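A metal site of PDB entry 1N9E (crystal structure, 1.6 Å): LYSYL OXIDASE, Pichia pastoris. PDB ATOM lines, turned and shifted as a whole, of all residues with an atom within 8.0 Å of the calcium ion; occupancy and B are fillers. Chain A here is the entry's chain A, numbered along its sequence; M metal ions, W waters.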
ATOM      1  N   GLU A 580     -32.585  21.118  24.286  1.00  0.00           N
ATOM      2  CA  GLU A 580     -33.030  19.811  23.810  1.00  0.00           C
ATOM      3  C   GLU A 580     -34.547  19.834  23.619  1.00  0.00           C
ATOM      4  O   GLU A 580     -35.295  20.370  24.452  1.00  0.00           O
ATOM      5  CB  GLU A 580     -32.620  18.709  24.805  1.00  0.00           C
ATOM      6  CG  GLU A 580     -31.125  18.510  24.895  1.00  0.00           C
ATOM      7  CD  GLU A 580     -30.739  17.604  26.054  1.00  0.00           C
ATOM      8  OE1 GLU A 580     -31.518  17.539  27.030  1.00  0.00           O
ATOM      9  OE2 GLU A 580     -29.667  16.960  26.003  1.00  0.00           O
ATOM     10  N   LEU A 644     -31.004  16.125  18.877  1.00  0.00           N
ATOM     11  CA  LEU A 644     -29.759  16.784  19.292  1.00  0.00           C
ATOM     12  C   LEU A 644     -29.737  16.754  20.814  1.00  0.00           C
ATOM     13  O   LEU A 644     -30.689  17.198  21.440  1.00  0.00           O
ATOM     14  CB  LEU A 644     -29.741  18.232  18.812  1.00  0.00           C
ATOM     15  CG  LEU A 644     -29.706  18.438  17.305  1.00  0.00           C
ATOM     16  CD1 LEU A 644     -29.817  19.932  17.009  1.00  0.00           C
ATOM     17  CD2 LEU A 644     -28.419  17.842  16.731  1.00  0.00           C
ATOM     18  N   THR A 645     -28.651  16.235  21.383  1.00  0.00           N
ATOM     19  CA  THR A 645     -28.505  16.217  22.844  1.00  0.00           C
ATOM     20  C   THR A 645     -27.171  16.762  23.293  1.00  0.00           C
ATOM     21  O   THR A 645     -26.205  16.888  22.513  1.00  0.00           O
ATOM     22  CB  THR A 645     -28.687  14.821  23.443  1.00  0.00           C
ATOM     23  OG1 THR A 645     -27.615  13.957  23.028  1.00  0.00           O
ATOM     24  CG2 THR A 645     -29.975  14.154  22.922  1.00  0.00           C
ATOM     25  N   LYS A 646     -27.111  17.085  24.572  1.00  0.00           N
ATOM     26  CA  LYS A 646     -25.838  17.449  25.196  1.00  0.00           C
ATOM     27  C   LYS A 646     -25.038  16.182  25.454  1.00  0.00           C
ATOM     28  O   LYS A 646     -25.536  15.228  26.077  1.00  0.00           O
ATOM     29  CB  LYS A 646     -26.097  18.173  26.528  1.00  0.00           C
ATOM     30  CG  LYS A 646     -24.845  18.518  27.320  1.00  0.00           C
ATOM     31  CD  LYS A 646     -25.331  19.084  28.704  1.00  0.00           C
ATOM     32  CE  LYS A 646     -24.208  19.486  29.624  1.00  0.00           C
ATOM     33  NZ  LYS A 646     -24.843  20.206  30.795  1.00  0.00           N
ATOM     34  N   HIS A 647     -23.792  16.154  24.969  1.00  0.00           N
ATOM     35  CA  HIS A 647     -22.958  14.997  25.194  1.00  0.00           C
ATOM     36  C   HIS A 647     -22.778  14.595  26.660  1.00  0.00           C
ATOM     37  O   HIS A 647     -22.528  15.447  27.520  1.00  0.00           O
ATOM     38  CB  HIS A 647     -21.553  15.192  24.623  1.00  0.00           C
ATOM     39  CG  HIS A 647     -20.676  14.012  24.873  1.00  0.00           C
ATOM     40  ND1 HIS A 647     -19.909  13.876  26.025  1.00  0.00           N
ATOM     41  CD2 HIS A 647     -20.431  12.918  24.122  1.00  0.00           C
ATOM     42  CE1 HIS A 647     -19.253  12.739  25.960  1.00  0.00           C
ATOM     43  NE2 HIS A 647     -19.543  12.139  24.825  1.00  0.00           N
ATOM     44  N   LYS A 648     -22.904  13.308  26.922  1.00  0.00           N
ATOM     45  CA  LYS A 648     -22.626  12.757  28.243  1.00  0.00           C
ATOM     46  C   LYS A 648     -22.019  11.360  28.129  1.00  0.00           C
ATOM     47  O   LYS A 648     -22.491  10.513  27.350  1.00  0.00           O
ATOM     48  CB  LYS A 648     -23.905  12.701  29.103  1.00  0.00           C
ATOM     49  CG  LYS A 648     -24.530  14.056  29.424  1.00  0.00           C
ATOM     50  CD  LYS A 648     -25.710  13.947  30.410  1.00  0.00           C
ATOM     51  CE  LYS A 648     -26.345  15.328  30.606  1.00  0.00           C
ATOM     52  NZ  LYS A 648     -27.551  15.312  31.478  1.00  0.00           N
ATOM     53  N   GLU A 651     -24.531   8.774  28.516  1.00  0.00           N
ATOM     54  CA  GLU A 651     -25.482   8.623  27.389  1.00  0.00           C
ATOM     55  C   GLU A 651     -24.598   8.167  26.236  1.00  0.00           C
ATOM     56  O   GLU A 651     -24.429   8.809  25.193  1.00  0.00           O
ATOM     57  CB  GLU A 651     -26.199   9.959  27.170  1.00  0.00           C
ATOM     58  CG  GLU A 651     -27.013  10.291  28.430  1.00  0.00           C
ATOM     59  CD  GLU A 651     -27.947  11.475  28.307  1.00  0.00           C
ATOM     60  OE1 GLU A 651     -27.940  12.138  27.265  1.00  0.00           O
ATOM     61  OE2 GLU A 651     -28.690  11.719  29.280  1.00  0.00           O
ATOM     62  N   PHE A 670     -34.110   5.830  25.477  1.00  0.00           N
ATOM     63  CA  PHE A 670     -33.526   6.976  24.788  1.00  0.00           C
ATOM     64  C   PHE A 670     -34.141   8.305  25.233  1.00  0.00           C
ATOM     65  O   PHE A 670     -33.471   9.347  25.276  1.00  0.00           O
ATOM     66  CB  PHE A 670     -33.660   6.803  23.261  1.00  0.00           C
ATOM     67  CG  PHE A 670     -33.130   7.978  22.483  1.00  0.00           C
ATOM     68  CD1 PHE A 670     -31.760   8.116  22.257  1.00  0.00           C
ATOM     69  CD2 PHE A 670     -34.003   8.944  21.987  1.00  0.00           C
ATOM     70  CE1 PHE A 670     -31.282   9.217  21.545  1.00  0.00           C
ATOM     71  CE2 PHE A 670     -33.527  10.036  21.281  1.00  0.00           C
ATOM     72  CZ  PHE A 670     -32.169  10.171  21.049  1.00  0.00           C
ATOM     73  N   ASN A 671     -35.424   8.288  25.574  1.00  0.00           N
ATOM     74  CA  ASN A 671     -36.092   9.525  25.949  1.00  0.00           C
ATOM     75  C   ASN A 671     -35.519  10.171  27.210  1.00  0.00           C
ATOM     76  O   ASN A 671     -35.674  11.381  27.423  1.00  0.00           O
ATOM     77  CB  ASN A 671     -37.602   9.301  26.127  1.00  0.00           C
ATOM     78  CG  ASN A 671     -38.342   9.153  24.805  1.00  0.00           C
ATOM     79  OD1 ASN A 671     -37.796   9.457  23.736  1.00  0.00           O
ATOM     80  ND2 ASN A 671     -39.587   8.682  24.886  1.00  0.00           N
ATOM     81  N   ALA A 672     -34.852   9.394  28.045  1.00  0.00           N
ATOM     82  CA  ALA A 672     -34.208   9.949  29.230  1.00  0.00           C
ATOM     83  C   ALA A 672     -33.129  10.986  28.884  1.00  0.00           C
ATOM     84  O   ALA A 672     -32.759  11.802  29.753  1.00  0.00           O
ATOM     85  CB  ALA A 672     -33.584   8.837  30.063  1.00  0.00           C
ATOM     86  N   PHE A 673     -32.605  10.957  27.657  1.00  0.00           N
ATOM     87  CA  PHE A 673     -31.559  11.897  27.236  1.00  0.00           C
ATOM     88  C   PHE A 673     -32.123  13.290  27.005  1.00  0.00           C
ATOM     89  O   PHE A 673     -31.379  14.287  27.041  1.00  0.00           O
ATOM     90  CB  PHE A 673     -30.942  11.501  25.883  1.00  0.00           C
ATOM     91  CG  PHE A 673     -30.223  10.167  25.853  1.00  0.00           C
ATOM     92  CD1 PHE A 673     -30.127   9.330  26.949  1.00  0.00           C
ATOM     93  CD2 PHE A 673     -29.627   9.760  24.662  1.00  0.00           C
ATOM     94  CE1 PHE A 673     -29.459   8.111  26.872  1.00  0.00           C
ATOM     95  CE2 PHE A 673     -28.951   8.551  24.564  1.00  0.00           C
ATOM     96  CZ  PHE A 673     -28.862   7.713  25.676  1.00  0.00           C
ATOM     97  N   LEU A 674     -33.427  13.357  26.753  1.00  0.00           N
ATOM     98  CA  LEU A 674     -34.119  14.574  26.357  1.00  0.00           C
ATOM     99  C   LEU A 674     -34.760  15.214  27.569  1.00  0.00           C
ATOM    100  O   LEU A 674     -35.895  14.882  27.957  1.00  0.00           O
ATOM    101  CB  LEU A 674     -35.199  14.233  25.333  1.00  0.00           C
ATOM    102  CG  LEU A 674     -34.644  13.473  24.114  1.00  0.00           C
ATOM    103  CD1 LEU A 674     -35.755  12.904  23.250  1.00  0.00           C
ATOM    104  CD2 LEU A 674     -33.770  14.414  23.303  1.00  0.00           C
ATOM    105  N   ASP A 675     -34.019  16.136  28.175  1.00  0.00           N
ATOM    106  CA  ASP A 675     -34.490  16.712  29.413  1.00  0.00           C
ATOM    107  C   ASP A 675     -34.224  18.225  29.427  1.00  0.00           C
ATOM    108  O   ASP A 675     -33.831  18.830  30.452  1.00  0.00           O
ATOM    109  CB  ASP A 675     -33.934  15.910  30.597  1.00  0.00           C
ATOM    110  CG  ASP A 675     -32.421  15.766  30.572  1.00  0.00           C
ATOM    111  OD1 ASP A 675     -31.870  15.027  31.419  1.00  0.00           O
ATOM    112  OD2 ASP A 675     -31.700  16.362  29.738  1.00  0.00           O
ATOM    113  N   ASP A 676     -34.443  18.824  28.254  1.00  0.00           N
ATOM    114  CA  ASP A 676     -34.500  20.262  28.076  1.00  0.00           C
ATOM    115  C   ASP A 676     -33.225  21.021  28.392  1.00  0.00           C
ATOM    116  O   ASP A 676     -33.267  22.224  28.710  1.00  0.00           O
ATOM    117  CB  ASP A 676     -35.669  20.812  28.914  1.00  0.00           C
ATOM    118  CG  ASP A 676     -37.006  20.262  28.456  1.00  0.00           C
ATOM    119  OD1 ASP A 676     -37.339  20.441  27.259  1.00  0.00           O
ATOM    120  OD2 ASP A 676     -37.781  19.634  29.204  1.00  0.00           O
ATOM    121  N   GLU A 677     -32.091  20.337  28.322  1.00  0.00           N
ATOM    122  CA  GLU A 677     -30.831  21.003  28.605  1.00  0.00           C
ATOM    123  C   GLU A 677     -30.447  21.968  27.504  1.00  0.00           C
ATOM    124  O   GLU A 677     -30.771  21.780  26.333  1.00  0.00           O
ATOM    125  CB  GLU A 677     -29.727  19.988  28.847  1.00  0.00           C
ATOM    126  CG  GLU A 677     -29.969  19.168  30.105  1.00  0.00           C
ATOM    127  CD  GLU A 677     -28.952  18.061  30.312  1.00  0.00           C
ATOM    128  OE1 GLU A 677     -28.718  17.276  29.374  1.00  0.00           O
ATOM    129  OE2 GLU A 677     -28.381  17.977  31.418  1.00  0.00           O
ATOM    130  N   SER A 678     -29.754  23.028  27.899  1.00  0.00           N
ATOM    131  CA  SER A 678     -29.246  23.972  26.920  1.00  0.00           C
ATOM    132  C   SER A 678     -28.295  23.292  25.942  1.00  0.00           C
ATOM    133  O   SER A 678     -27.490  22.455  26.338  1.00  0.00           O
ATOM    134  CB  SER A 678     -28.477  25.087  27.638  1.00  0.00           C
ATOM    135  OG  SER A 678     -27.924  25.999  26.703  1.00  0.00           O
ATOM    136  N   LEU A 679     -28.403  23.649  24.667  1.00  0.00           N
ATOM    137  CA  LEU A 679     -27.443  23.214  23.662  1.00  0.00           C
ATOM    138  C   LEU A 679     -26.666  24.415  23.158  1.00  0.00           C
ATOM    139  O   LEU A 679     -25.894  24.318  22.192  1.00  0.00           O
ATOM    140  CB  LEU A 679     -28.193  22.586  22.484  1.00  0.00           C
ATOM    141  CG  LEU A 679     -29.011  21.345  22.817  1.00  0.00           C
ATOM    142  CD1 LEU A 679     -29.835  20.907  21.613  1.00  0.00           C
ATOM    143  CD2 LEU A 679     -28.075  20.220  23.260  1.00  0.00           C
HETATM  144 CA    CA M   1     -29.989  15.896  28.113  1.00  0.00          CA
HETATM  145  O   HOH W   1     -28.045  14.861  27.403  1.00  0.00           O
HETATM  146  O   HOH W   2     -29.652  14.206  29.862  1.00  0.00           O
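OE2 of Glu 677 lies within salt-bridge range of NZ of Lys 648, at 2.8 Å. OE2 of Glu 580 lies close to N of Lys 646 (2.9 Å). The side-chain carboxylate (OE1) of Glu 580 lies close to the backbone NH (N) of Asp 676 (3.4 Å).
Four residues have an atom within 4 Å of the calcium ion: Glu 580, Phe 673, Asp 675 and Glu 677.
The calcium ion is bound by the side-chain carboxylate (OE1) of Glu 677 (2.3 Å), water W1 (2.3 Å), the backbone carbonyl oxygen (O) of Phe 673 (2.4 Å), the side-chain carboxylate (OE2) of Glu 580 (2.4 Å), the side-chain carboxylate (OD2) of Asp 675 (2.4 Å), water W2 (2.5 Å) and the side-chain carboxylate (OE1) of Glu 580 (2.5 Å). The calcium ion has seven donor atoms within binding distance.
Water W1 lies within hydrogen-bond range of the side-chain carboxylate (OE1) of Glu 651 (2.7 Å) and the backbone carbonyl oxygen (O) of Lys 646 (2.9 Å). Water W2 lies within hydrogen-bond range of the side-chain carboxylate (OE2) of Glu 651 (2.7 Å), the side-chain carboxylate (OD1) of Asp 675 (2.8 Å) and the side-chain amino group (NZ) of Lys 648 (2.9 Å).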
